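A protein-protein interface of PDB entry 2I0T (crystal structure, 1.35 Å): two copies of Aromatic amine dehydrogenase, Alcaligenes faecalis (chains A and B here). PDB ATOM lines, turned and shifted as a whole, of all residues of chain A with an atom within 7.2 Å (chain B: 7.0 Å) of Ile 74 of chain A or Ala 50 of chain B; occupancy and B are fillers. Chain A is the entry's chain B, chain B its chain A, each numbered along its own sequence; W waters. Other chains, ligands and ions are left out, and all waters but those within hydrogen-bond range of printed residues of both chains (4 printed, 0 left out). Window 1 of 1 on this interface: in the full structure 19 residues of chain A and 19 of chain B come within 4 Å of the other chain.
Of the printed residues of chain B, Thr 29 of chain A touches Glu 30. Of the printed residues of chain B, Arg 73 of chain A touches Tyr 70 (3.4 Å). Ile 74 of chain A touches just these residues of chain B: Ala 50 (3.6 Å) and Tyr 70 (3.9 Å). Printed residues of chain A within 4 Å of Glu 30 of chain B: Thr 29. Of the printed residues of chain A, Ala 50 of chain B touches Ile 74 (3.6 Å). The nearest printed residue of chain A that does not touch Ile 74 of chain B is Thr 29 of chain A (4.6 Å).
Tyr 70 of chain A touches Ile 74 of chain B, and with the chains exchanged Ile 74 of chain A touches Tyr 70 of chain B. Of the 7 pairs that touch across the chains among the printed residues, 2 have their exchanged pair printed and touching as well.
Of the 23 printed residues of chain B, 6 touch a printed residue of chain A. Hydrophobic or aromatic side chains of chain A within 4 Å of the printed part of chain B: Tyr 70 and Ile 74. Among the printed residues, Asp or Glu carboxylates within 4 Å of a Lys or Arg side-chain nitrogen of the other chain: Arg 76 of chain A with Glu 84 of chain B.
Water W1 bridges O of Thr 29 of chain A (2.7 Å) and OG1 of Thr 29 of chain B (2.8 Å). Water W3 bridges the backbone carbonyl oxygen of Thr 29 of chain B (2.7 Å) and the side-chain hydroxyl of Thr 29 of chain A (2.8 Å). Water W2 lies within hydrogen-bond range of OE1 of Glu 84 of chain B (2.8 Å), NE of Arg 76 of chain A (2.9 Å) and OH of Tyr 70 of chain B (3.2 Å). Water W4 lies within hydrogen-bond range of the backbone carbonyl oxygen (O) of His 71 of chain B (3.0 Å) and the backbone carbonyl oxygen (O) of His 71 of chain A (3.0 Å).
The side-chain carboxylate (OE1) of Glu 30 of chain B lies within hydrogen-bond range of the side-chain hydroxyl (OG1) of Thr 29 of chain A, 2.6 Å away. OE2 of Glu 84 of chain B lies within salt-bridge range of NH2 of Arg 76 of chain A, at 2.9 Å.
Tyr 70 of chain A touches Ile 74 of chain B. Arg 73 of chain A touches Tyr 70 of chain B. Ile 74 of chain A touches Ala 50 of chain B. CD1 of Ile 74 of chain A touches CE2 of Tyr 70 of chain B, 3.9 Å away. Thr 75 of chain A touches Pro 48 of chain B.
The side-chain hydroxyl (OH) of Tyr 70 of chain B sits at hydrogen-bond distance from the side-chain carboxylate (OE2) of Glu 84 of chain B (2.6 Å). A ring nitrogen (ND1) of His 71 of chain B is in hydrogen-bond range of the backbone carbonyl oxygen (O) of Ile 74 of chain B (3.3 Å). The guanidinium group (NH2) of Arg 32 of chain B is in salt-bridge range of the side-chain carboxylate (OE2) of Glu 30 of chain B. OG of Ser 31 of chain B lies within hydrogen-bond range of O of Ala 50 of chain B.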
ATOM      1  N   THR A  29     -30.155 -18.603  -7.065  1.00  0.00           N
ATOM      2  CA  THR A  29     -28.884 -17.945  -6.783  1.00  0.00           C
ATOM      3  C   THR A  29     -27.689 -18.874  -6.875  1.00  0.00           C
ATOM      4  O   THR A  29     -26.572 -18.402  -6.734  1.00  0.00           O
ATOM      5  CB  THR A  29     -28.848 -17.261  -5.397  1.00  0.00           C
ATOM      6  OG1 THR A  29     -28.947 -18.225  -4.352  1.00  0.00           O
ATOM      7  CG2 THR A  29     -29.914 -16.200  -5.269  1.00  0.00           C
ATOM      8  N   PHE A  51     -26.691 -16.008  -9.635  1.00  0.00           N
ATOM      9  CA  PHE A  51     -28.123 -15.873  -9.868  1.00  0.00           C
ATOM     10  C   PHE A  51     -28.458 -15.943 -11.347  1.00  0.00           C
ATOM     11  O   PHE A  51     -28.038 -15.080 -12.109  1.00  0.00           O
ATOM     12  CB  PHE A  51     -28.662 -14.553  -9.308  1.00  0.00           C
ATOM     13  CG  PHE A  51     -30.125 -14.358  -9.540  1.00  0.00           C
ATOM     14  CD1 PHE A  51     -31.053 -15.030  -8.784  1.00  0.00           C
ATOM     15  CD2 PHE A  51     -30.568 -13.493 -10.515  1.00  0.00           C
ATOM     16  CE1 PHE A  51     -32.384 -14.852  -9.003  1.00  0.00           C
ATOM     17  CE2 PHE A  51     -31.917 -13.313 -10.737  1.00  0.00           C
ATOM     18  CZ  PHE A  51     -32.818 -13.982  -9.969  1.00  0.00           C
ATOM     19  N   THR A  69     -25.501 -12.191 -12.305  1.00  0.00           N
ATOM     20  CA  THR A  69     -25.754 -11.054 -11.404  1.00  0.00           C
ATOM     21  C   THR A  69     -25.325 -11.433 -10.015  1.00  0.00           C
ATOM     22  O   THR A  69     -25.688 -12.495  -9.540  1.00  0.00           O
ATOM     23  CB  THR A  69     -27.228 -10.692 -11.369  1.00  0.00           C
ATOM     24  OG1 THR A  69     -27.616 -10.216 -12.648  1.00  0.00           O
ATOM     25  CG2 THR A  69     -27.529  -9.602 -10.348  1.00  0.00           C
ATOM     26  N   TYR A  70     -24.530 -10.567  -9.392  1.00  0.00           N
ATOM     27  CA  TYR A  70     -24.167 -10.650  -7.997  1.00  0.00           C
ATOM     28  C   TYR A  70     -24.766  -9.458  -7.251  1.00  0.00           C
ATOM     29  O   TYR A  70     -25.025  -8.395  -7.844  1.00  0.00           O
ATOM     30  CB  TYR A  70     -22.640 -10.574  -7.839  1.00  0.00           C
ATOM     31  CG  TYR A  70     -21.855 -11.686  -8.492  1.00  0.00           C
ATOM     32  CD1 TYR A  70     -21.364 -11.563  -9.777  1.00  0.00           C
ATOM     33  CD2 TYR A  70     -21.638 -12.876  -7.835  1.00  0.00           C
ATOM     34  CE1 TYR A  70     -20.622 -12.561 -10.371  1.00  0.00           C
ATOM     35  CE2 TYR A  70     -20.909 -13.895  -8.424  1.00  0.00           C
ATOM     36  CZ  TYR A  70     -20.408 -13.727  -9.705  1.00  0.00           C
ATOM     37  OH  TYR A  70     -19.666 -14.754 -10.264  1.00  0.00           O
ATOM     38  N   HIS A  71     -24.914  -9.619  -5.938  1.00  0.00           N
ATOM     39  CA  HIS A  71     -25.091  -8.457  -5.061  1.00  0.00           C
ATOM     40  C   HIS A  71     -24.168  -8.645  -3.871  1.00  0.00           C
ATOM     41  O   HIS A  71     -23.857  -9.758  -3.485  1.00  0.00           O
ATOM     42  CB  HIS A  71     -26.517  -8.277  -4.554  1.00  0.00           C
ATOM     43  CG  HIS A  71     -27.524  -8.089  -5.625  1.00  0.00           C
ATOM     44  ND1 HIS A  71     -28.082  -6.873  -5.958  1.00  0.00           N
ATOM     45  CD2 HIS A  71     -28.100  -8.997  -6.437  1.00  0.00           C
ATOM     46  CE1 HIS A  71     -28.969  -7.051  -6.928  1.00  0.00           C
ATOM     47  NE2 HIS A  71     -28.993  -8.333  -7.230  1.00  0.00           N
ATOM     48  N   GLU A  72     -23.799  -7.528  -3.246  1.00  0.00           N
ATOM     49  CA  GLU A  72     -22.821  -7.573  -2.155  1.00  0.00           C
ATOM     50  C   GLU A  72     -23.224  -8.532  -1.036  1.00  0.00           C
ATOM     51  O   GLU A  72     -22.388  -9.182  -0.410  1.00  0.00           O
ATOM     52  CB  GLU A  72     -22.582  -6.182  -1.551  1.00  0.00           C
ATOM     53  CG  GLU A  72     -22.072  -5.103  -2.468  1.00  0.00           C
ATOM     54  CD  GLU A  72     -22.086  -3.699  -1.813  1.00  0.00           C
ATOM     55  OE1 GLU A  72     -23.173  -3.180  -1.398  1.00  0.00           O
ATOM     56  OE2 GLU A  72     -20.991  -3.094  -1.747  1.00  0.00           O
ATOM     57  N   ARG A  73     -24.538  -8.604  -0.783  1.00  0.00           N
ATOM     58  CA  ARG A  73     -25.067  -9.500   0.224  1.00  0.00           C
ATOM     59  C   ARG A  73     -26.211 -10.356  -0.333  1.00  0.00           C
ATOM     60  O   ARG A  73     -27.102 -10.752   0.412  1.00  0.00           O
ATOM     61  CB  ARG A  73     -25.517  -8.690   1.453  1.00  0.00           C
ATOM     62  CG  ARG A  73     -24.369  -7.994   2.158  1.00  0.00           C
ATOM     63  CD  ARG A  73     -23.564  -8.987   2.963  1.00  0.00           C
ATOM     64  NE  ARG A  73     -22.541  -8.361   3.785  1.00  0.00           N
ATOM     65  CZ  ARG A  73     -21.308  -8.101   3.396  1.00  0.00           C
ATOM     66  NH1 ARG A  73     -20.888  -8.385   2.180  1.00  0.00           N
ATOM     67  NH2 ARG A  73     -20.478  -7.510   4.248  1.00  0.00           N
ATOM     68  N   ILE A  74     -26.133 -10.643  -1.635  1.00  0.00           N
ATOM     69  CA  ILE A  74     -27.027 -11.560  -2.377  1.00  0.00           C
ATOM     70  C   ILE A  74     -28.439 -10.972  -2.546  1.00  0.00           C
ATOM     71  O   ILE A  74     -28.849 -10.656  -3.667  1.00  0.00           O
ATOM     72  CB  ILE A  74     -27.056 -12.992  -1.789  1.00  0.00           C
ATOM     73  CG1 ILE A  74     -25.642 -13.542  -1.585  1.00  0.00           C
ATOM     74  CG2 ILE A  74     -27.866 -13.863  -2.723  1.00  0.00           C
ATOM     75  CD1 ILE A  74     -25.602 -14.745  -0.752  1.00  0.00           C
ATOM     76  N   THR A  75     -29.181 -10.870  -1.439  1.00  0.00           N
ATOM     77  CA  THR A  75     -30.531 -10.369  -1.401  1.00  0.00           C
ATOM     78  C   THR A  75     -30.590  -8.889  -1.003  1.00  0.00           C
ATOM     79  O   THR A  75     -31.685  -8.323  -0.948  1.00  0.00           O
ATOM     80  CB  THR A  75     -31.373 -11.207  -0.477  1.00  0.00           C
ATOM     81  OG1 THR A  75     -30.668 -11.378   0.758  1.00  0.00           O
ATOM     82  CG2 THR A  75     -31.650 -12.562  -1.116  1.00  0.00           C
ATOM     83  N   ARG A  76     -29.439  -8.277  -0.754  1.00  0.00           N
ATOM     84  CA  ARG A  76     -29.351  -6.840  -0.541  1.00  0.00           C
ATOM     85  C   ARG A  76     -27.960  -6.391  -0.983  1.00  0.00           C
ATOM     86  O   ARG A  76     -27.079  -7.210  -1.237  1.00  0.00           O
ATOM     87  CB  ARG A  76     -29.640  -6.485   0.924  1.00  0.00           C
ATOM     88  CG  ARG A  76     -28.646  -7.050   1.888  1.00  0.00           C
ATOM     89  CD  ARG A  76     -29.027  -6.831   3.356  1.00  0.00           C
ATOM     90  NE  ARG A  76     -28.142  -7.558   4.231  1.00  0.00           N
ATOM     91  CZ  ARG A  76     -26.973  -7.126   4.663  1.00  0.00           C
ATOM     92  NH1 ARG A  76     -26.558  -5.907   4.354  1.00  0.00           N
ATOM     93  NH2 ARG A  76     -26.231  -7.933   5.385  1.00  0.00           N
ATOM     94  N   GLY A  77     -27.760  -5.089  -1.048  1.00  0.00           N
ATOM     95  CA  GLY A  77     -26.462  -4.532  -1.416  1.00  0.00           C
ATOM     96  C   GLY A  77     -26.359  -4.269  -2.898  1.00  0.00           C
ATOM     97  O   GLY A  77     -27.253  -4.549  -3.680  1.00  0.00           O
ATOM     98  N   LYS A  78     -25.217  -3.725  -3.294  1.00  0.00           N
ATOM     99  CA  LYS A  78     -25.064  -3.240  -4.645  1.00  0.00           C
ATOM    100  C   LYS A  78     -25.022  -4.391  -5.651  1.00  0.00           C
ATOM    101  O   LYS A  78     -24.401  -5.405  -5.390  1.00  0.00           O
ATOM    102  CB  LYS A  78     -23.788  -2.427  -4.777  1.00  0.00           C
ATOM    103  CG  LYS A  78     -23.686  -1.758  -6.124  1.00  0.00           C
ATOM    104  CD  LYS A  78     -22.446  -0.933  -6.243  1.00  0.00           C
ATOM    105  CE  LYS A  78     -22.452  -0.104  -7.518  1.00  0.00           C
ATOM    106  NZ  LYS A  78     -21.059   0.255  -7.858  1.00  0.00           N
ATOM    107  N   MET B  21     -34.424 -24.620  10.076  1.00  0.00           N
ATOM    108  CA  MET B  21     -33.204 -24.126   9.466  1.00  0.00           C
ATOM    109  C   MET B  21     -32.839 -25.041   8.310  1.00  0.00           C
ATOM    110  O   MET B  21     -32.405 -26.180   8.550  1.00  0.00           O
ATOM    111  CB  MET B  21     -32.090 -24.064  10.503  1.00  0.00           C
ATOM    112  CG  MET B  21     -30.738 -23.577   9.978  1.00  0.00           C
ATOM    113  SD  MET B  21     -30.771 -21.886   9.365  1.00  0.00           S
ATOM    114  CE  MET B  21     -30.203 -22.114   7.690  1.00  0.00           C
ATOM    115  N   ASP B  22     -33.059 -24.593   7.080  1.00  0.00           N
ATOM    116  CA  ASP B  22     -32.829 -25.441   5.915  1.00  0.00           C
ATOM    117  C   ASP B  22     -31.416 -25.181   5.388  1.00  0.00           C
ATOM    118  O   ASP B  22     -31.153 -24.140   4.819  1.00  0.00           O
ATOM    119  CB  ASP B  22     -33.874 -25.226   4.850  1.00  0.00           C
ATOM    120  CG  ASP B  22     -33.902 -26.342   3.813  1.00  0.00           C
ATOM    121  OD1 ASP B  22     -32.988 -27.184   3.828  1.00  0.00           O
ATOM    122  OD2 ASP B  22     -34.834 -26.357   2.975  1.00  0.00           O
ATOM    123  N   SER B  23     -30.519 -26.125   5.610  1.00  0.00           N
ATOM    124  CA  SER B  23     -29.151 -25.984   5.117  1.00  0.00           C
ATOM    125  C   SER B  23     -29.130 -25.995   3.601  1.00  0.00           C
ATOM    126  O   SER B  23     -28.242 -25.421   3.006  1.00  0.00           O
ATOM    127  CB  SER B  23     -28.257 -27.081   5.675  1.00  0.00           C
ATOM    128  OG  SER B  23     -28.475 -28.327   5.016  1.00  0.00           O
ATOM    129  N   HIS B  27     -27.375 -27.133  -2.327  1.00  0.00           N
ATOM    130  CA  HIS B  27     -27.130 -25.778  -2.788  1.00  0.00           C
ATOM    131  C   HIS B  27     -26.882 -24.919  -1.583  1.00  0.00           C
ATOM    132  O   HIS B  27     -27.623 -23.974  -1.315  1.00  0.00           O
ATOM    133  CB  HIS B  27     -28.294 -25.286  -3.648  1.00  0.00           C
ATOM    134  CG  HIS B  27     -28.501 -26.134  -4.853  1.00  0.00           C
ATOM    135  ND1 HIS B  27     -27.586 -26.172  -5.890  1.00  0.00           N
ATOM    136  CD2 HIS B  27     -29.445 -27.058  -5.144  1.00  0.00           C
ATOM    137  CE1 HIS B  27     -27.971 -27.085  -6.770  1.00  0.00           C
ATOM    138  NE2 HIS B  27     -29.092 -27.636  -6.343  1.00  0.00           N
ATOM    139  N   LEU B  28     -25.795 -25.216  -0.888  1.00  0.00           N
ATOM    140  CA  LEU B  28     -25.559 -24.729   0.473  1.00  0.00           C
ATOM    141  C   LEU B  28     -25.327 -23.223   0.522  1.00  0.00           C
ATOM    142  O   LEU B  28     -25.395 -22.624   1.615  1.00  0.00           O
ATOM    143  CB  LEU B  28     -24.338 -25.459   1.035  1.00  0.00           C
ATOM    144  CG  LEU B  28     -23.956 -25.229   2.485  1.00  0.00           C
ATOM    145  CD1 LEU B  28     -25.127 -25.461   3.450  1.00  0.00           C
ATOM    146  CD2 LEU B  28     -22.790 -26.126   2.886  1.00  0.00           C
ATOM    147  N   THR B  29     -25.053 -22.582  -0.620  1.00  0.00           N
ATOM    148  CA  THR B  29     -25.008 -21.123  -0.673  1.00  0.00           C
ATOM    149  C   THR B  29     -26.384 -20.462  -0.593  1.00  0.00           C
ATOM    150  O   THR B  29     -26.456 -19.223  -0.517  1.00  0.00           O
ATOM    151  CB  THR B  29     -24.268 -20.569  -1.899  1.00  0.00           C
ATOM    152  OG1 THR B  29     -25.006 -20.851  -3.090  1.00  0.00           O
ATOM    153  CG2 THR B  29     -22.851 -21.098  -1.979  1.00  0.00           C
ATOM    154  N   GLU B  30     -27.477 -21.230  -0.660  1.00  0.00           N
ATOM    155  CA  GLU B  30     -28.846 -20.675  -0.576  1.00  0.00           C
ATOM    156  C   GLU B  30     -29.608 -21.310   0.575  1.00  0.00           C
ATOM    157  O   GLU B  30     -30.829 -21.521   0.496  1.00  0.00           O
ATOM    158  CB  GLU B  30     -29.594 -20.767  -1.896  1.00  0.00           C
ATOM    159  CG  GLU B  30     -30.618 -19.650  -2.005  1.00  0.00           C
ATOM    160  CD  GLU B  30     -31.547 -19.841  -3.163  1.00  0.00           C
ATOM    161  OE1 GLU B  30     -31.259 -19.371  -4.290  1.00  0.00           O
ATOM    162  OE2 GLU B  30     -32.612 -20.464  -2.950  1.00  0.00           O
ATOM    163  N   SER B  31     -28.900 -21.503   1.683  1.00  0.00           N
ATOM    164  CA  SER B  31     -29.538 -21.914   2.919  1.00  0.00           C
ATOM    165  C   SER B  31     -30.544 -20.852   3.355  1.00  0.00           C
ATOM    166  O   SER B  31     -30.436 -19.684   2.985  1.00  0.00           O
ATOM    167  CB  SER B  31     -28.499 -22.142   4.033  1.00  0.00           C
ATOM    168  OG  SER B  31     -27.878 -20.949   4.497  1.00  0.00           O
ATOM    169  N   ARG B  32     -31.521 -21.244   4.151  1.00  0.00           N
ATOM    170  CA  ARG B  32     -32.509 -20.280   4.625  1.00  0.00           C
ATOM    171  C   ARG B  32     -33.228 -20.857   5.820  1.00  0.00           C
ATOM    172  O   ARG B  32     -33.224 -22.047   6.044  1.00  0.00           O
ATOM    173  CB  ARG B  32     -33.533 -19.947   3.530  1.00  0.00           C
ATOM    174  CG  ARG B  32     -34.530 -21.053   3.172  1.00  0.00           C
ATOM    175  CD  ARG B  32     -34.010 -22.088   2.143  1.00  0.00           C
ATOM    176  NE  ARG B  32     -33.858 -21.489   0.824  1.00  0.00           N
ATOM    177  CZ  ARG B  32     -34.882 -21.165   0.018  1.00  0.00           C
ATOM    178  NH1 ARG B  32     -36.115 -21.391   0.393  1.00  0.00           N
ATOM    179  NH2 ARG B  32     -34.666 -20.561  -1.134  1.00  0.00           N
ATOM    180  N   VAL B  47     -36.295 -16.444   5.992  1.00  0.00           N
ATOM    181  CA  VAL B  47     -35.140 -15.537   6.060  1.00  0.00           C
ATOM    182  C   VAL B  47     -33.970 -16.179   5.291  1.00  0.00           C
ATOM    183  O   VAL B  47     -33.554 -17.302   5.623  1.00  0.00           O
ATOM    184  CB  VAL B  47     -34.709 -15.253   7.492  1.00  0.00           C
ATOM    185  CG1 VAL B  47     -33.507 -14.341   7.510  1.00  0.00           C
ATOM    186  CG2 VAL B  47     -35.899 -14.631   8.264  1.00  0.00           C
ATOM    187  N   PRO B  48     -33.435 -15.499   4.263  1.00  0.00           N
ATOM    188  CA  PRO B  48     -32.305 -16.057   3.506  1.00  0.00           C
ATOM    189  C   PRO B  48     -31.049 -15.984   4.348  1.00  0.00           C
ATOM    190  O   PRO B  48     -30.837 -14.979   5.048  1.00  0.00           O
ATOM    191  CB  PRO B  48     -32.211 -15.120   2.309  1.00  0.00           C
ATOM    192  CG  PRO B  48     -32.742 -13.818   2.812  1.00  0.00           C
ATOM    193  CD  PRO B  48     -33.857 -14.181   3.763  1.00  0.00           C
ATOM    194  N   THR B  49     -30.205 -17.028   4.299  1.00  0.00           N
ATOM    195  CA  THR B  49     -29.022 -17.094   5.113  1.00  0.00           C
ATOM    196  C   THR B  49     -27.765 -17.561   4.351  1.00  0.00           C
ATOM    197  O   THR B  49     -26.830 -18.043   4.967  1.00  0.00           O
ATOM    198  CB  THR B  49     -29.258 -17.967   6.348  1.00  0.00           C
ATOM    199  OG1 THR B  49     -29.619 -19.291   5.983  1.00  0.00           O
ATOM    200  CG2 THR B  49     -30.337 -17.409   7.234  1.00  0.00           C
ATOM    201  N   ALA B  50     -27.728 -17.336   3.034  1.00  0.00           N
ATOM    202  CA  ALA B  50     -26.497 -17.453   2.258  1.00  0.00           C
ATOM    203  C   ALA B  50     -25.825 -18.800   2.503  1.00  0.00           C
ATOM    204  O   ALA B  50     -26.487 -19.848   2.514  1.00  0.00           O
ATOM    205  CB  ALA B  50     -25.564 -16.230   2.492  1.00  0.00           C
ATOM    206  N   PHE B  51     -24.504 -18.804   2.700  1.00  0.00           N
ATOM    207  CA  PHE B  51     -23.785 -20.057   2.814  1.00  0.00           C
ATOM    208  C   PHE B  51     -23.877 -20.610   4.215  1.00  0.00           C
ATOM    209  O   PHE B  51     -23.361 -20.025   5.145  1.00  0.00           O
ATOM    210  CB  PHE B  51     -22.305 -19.885   2.423  1.00  0.00           C
ATOM    211  CG  PHE B  51     -21.514 -21.176   2.493  1.00  0.00           C
ATOM    212  CD1 PHE B  51     -21.678 -22.160   1.546  1.00  0.00           C
ATOM    213  CD2 PHE B  51     -20.624 -21.396   3.520  1.00  0.00           C
ATOM    214  CE1 PHE B  51     -20.983 -23.340   1.629  1.00  0.00           C
ATOM    215  CE2 PHE B  51     -19.915 -22.602   3.605  1.00  0.00           C
ATOM    216  CZ  PHE B  51     -20.075 -23.536   2.651  1.00  0.00           C
ATOM    217  N   ASN B  52     -24.464 -21.788   4.363  1.00  0.00           N
ATOM    218  CA  ASN B  52     -24.464 -22.522   5.625  1.00  0.00           C
ATOM    219  C   ASN B  52     -24.869 -21.624   6.803  1.00  0.00           C
ATOM    220  O   ASN B  52     -24.146 -21.480   7.780  1.00  0.00           O
ATOM    221  CB  ASN B  52     -23.087 -23.156   5.852  1.00  0.00           C
ATOM    222  CG  ASN B  52     -22.964 -23.913   7.181  1.00  0.00           C
ATOM    223  OD1 ASN B  52     -21.950 -23.779   7.869  1.00  0.00           O
ATOM    224  ND2 ASN B  52     -23.942 -24.730   7.548  1.00  0.00           N
ATOM    225  N   GLY B  53     -26.051 -21.047   6.707  1.00  0.00           N
ATOM    226  CA  GLY B  53     -26.545 -20.194   7.767  1.00  0.00           C
ATOM    227  C   GLY B  53     -26.843 -20.960   9.025  1.00  0.00           C
ATOM    228  O   GLY B  53     -27.146 -22.146   8.982  1.00  0.00           O
ATOM    229  N   THR B  68     -23.771 -16.150   9.108  1.00  0.00           N
ATOM    230  CA  THR B  68     -23.492 -16.651   7.768  1.00  0.00           C
ATOM    231  C   THR B  68     -22.179 -16.118   7.258  1.00  0.00           C
ATOM    232  O   THR B  68     -21.494 -15.352   7.944  1.00  0.00           O
ATOM    233  CB  THR B  68     -24.667 -16.368   6.832  1.00  0.00           C
ATOM    234  OG1 THR B  68     -24.451 -17.093   5.614  1.00  0.00           O
ATOM    235  CG2 THR B  68     -24.789 -14.904   6.499  1.00  0.00           C
ATOM    236  N   THR B  69     -21.827 -16.586   6.058  1.00  0.00           N
ATOM    237  CA  THR B  69     -20.624 -16.175   5.341  1.00  0.00           C
ATOM    238  C   THR B  69     -21.017 -15.725   3.965  1.00  0.00           C
ATOM    239  O   THR B  69     -21.731 -16.415   3.259  1.00  0.00           O
ATOM    240  CB  THR B  69     -19.643 -17.341   5.221  1.00  0.00           C
ATOM    241  OG1 THR B  69     -19.185 -17.695   6.526  1.00  0.00           O
ATOM    242  CG2 THR B  69     -18.450 -17.007   4.314  1.00  0.00           C
ATOM    243  N   TYR B  70     -20.521 -14.558   3.581  1.00  0.00           N
ATOM    244  CA  TYR B  70     -20.580 -14.048   2.223  1.00  0.00           C
ATOM    245  C   TYR B  70     -19.179 -13.974   1.640  1.00  0.00           C
ATOM    246  O   TYR B  70     -18.198 -13.868   2.363  1.00  0.00           O
ATOM    247  CB  TYR B  70     -21.141 -12.623   2.234  1.00  0.00           C
ATOM    248  CG  TYR B  70     -22.544 -12.482   2.757  1.00  0.00           C
ATOM    249  CD1 TYR B  70     -22.784 -12.143   4.077  1.00  0.00           C
ATOM    250  CD2 TYR B  70     -23.633 -12.726   1.946  1.00  0.00           C
ATOM    251  CE1 TYR B  70     -24.072 -12.002   4.559  1.00  0.00           C
ATOM    252  CE2 TYR B  70     -24.940 -12.604   2.428  1.00  0.00           C
ATOM    253  CZ  TYR B  70     -25.145 -12.230   3.739  1.00  0.00           C
ATOM    254  OH  TYR B  70     -26.432 -12.059   4.238  1.00  0.00           O
ATOM    255  N   HIS B  71     -19.120 -13.976   0.307  1.00  0.00           N
ATOM    256  CA  HIS B  71     -17.935 -13.520  -0.420  1.00  0.00           C
ATOM    257  C   HIS B  71     -18.377 -12.568  -1.504  1.00  0.00           C
ATOM    258  O   HIS B  71     -19.481 -12.673  -2.025  1.00  0.00           O
ATOM    259  CB  HIS B  71     -17.198 -14.710  -1.044  1.00  0.00           C
ATOM    260  CG  HIS B  71     -16.583 -15.640  -0.061  1.00  0.00           C
ATOM    261  ND1 HIS B  71     -17.279 -16.676   0.531  1.00  0.00           N
ATOM    262  CD2 HIS B  71     -15.321 -15.709   0.422  1.00  0.00           C
ATOM    263  CE1 HIS B  71     -16.457 -17.344   1.317  1.00  0.00           C
ATOM    264  NE2 HIS B  71     -15.268 -16.767   1.291  1.00  0.00           N
ATOM    265  N   ILE B  74     -19.105 -14.824  -4.206  1.00  0.00           N
ATOM    266  CA  ILE B  74     -19.604 -16.120  -3.715  1.00  0.00           C
ATOM    267  C   ILE B  74     -18.505 -17.170  -3.605  1.00  0.00           C
ATOM    268  O   ILE B  74     -18.144 -17.585  -2.512  1.00  0.00           O
ATOM    269  CB  ILE B  74     -20.814 -16.630  -4.521  1.00  0.00           C
ATOM    270  CG1 ILE B  74     -21.922 -15.560  -4.601  1.00  0.00           C
ATOM    271  CG2 ILE B  74     -21.347 -17.907  -3.874  1.00  0.00           C
ATOM    272  CD1 ILE B  74     -22.923 -15.843  -5.641  1.00  0.00           C
ATOM    273  N   GLU B  84     -26.405 -11.324  11.491  1.00  0.00           N
ATOM    274  CA  GLU B  84     -27.436 -10.381  11.109  1.00  0.00           C
ATOM    275  C   GLU B  84     -28.576 -10.410  12.101  1.00  0.00           C
ATOM    276  O   GLU B  84     -28.957 -11.470  12.626  1.00  0.00           O
ATOM    277  CB  GLU B  84     -27.971 -10.642   9.710  1.00  0.00           C
ATOM    278  CG  GLU B  84     -26.867 -10.660   8.656  1.00  0.00           C
ATOM    279  CD  GLU B  84     -27.343 -10.850   7.266  1.00  0.00           C
ATOM    280  OE1 GLU B  84     -28.530 -11.158   7.027  1.00  0.00           O
ATOM    281  OE2 GLU B  84     -26.522 -10.623   6.354  1.00  0.00           O
ATOM    282  N   ARG B 103     -16.015 -17.908  11.786  1.00  0.00           N
ATOM    283  CA  ARG B 103     -17.219 -18.458  12.381  1.00  0.00           C
ATOM    284  C   ARG B 103     -17.381 -19.903  11.932  1.00  0.00           C
ATOM    285  O   ARG B 103     -17.025 -20.270  10.810  1.00  0.00           O
ATOM    286  CB  ARG B 103     -18.455 -17.625  12.046  1.00  0.00           C
ATOM    287  CG  ARG B 103     -18.947 -17.716  10.618  1.00  0.00           C
ATOM    288  CD  ARG B 103     -19.909 -18.889  10.354  1.00  0.00           C
ATOM    289  NE  ARG B 103     -20.368 -18.890   8.985  1.00  0.00           N
ATOM    290  CZ  ARG B 103     -21.233 -19.753   8.496  1.00  0.00           C
ATOM    291  NH1 ARG B 103     -21.719 -20.720   9.251  1.00  0.00           N
ATOM    292  NH2 ARG B 103     -21.610 -19.634   7.243  1.00  0.00           N
HETATM  293  O   HOH W   1     -24.460 -19.107  -5.156  1.00  0.00           O
HETATM  294  O   HOH W   2     -29.124 -10.318   4.445  1.00  0.00           O
HETATM  295  O   HOH W   3     -27.799 -17.349  -1.978  1.00  0.00           O
HETATM  296  O   HOH W   4     -22.319 -12.276  -2.872  1.00  0.00           O
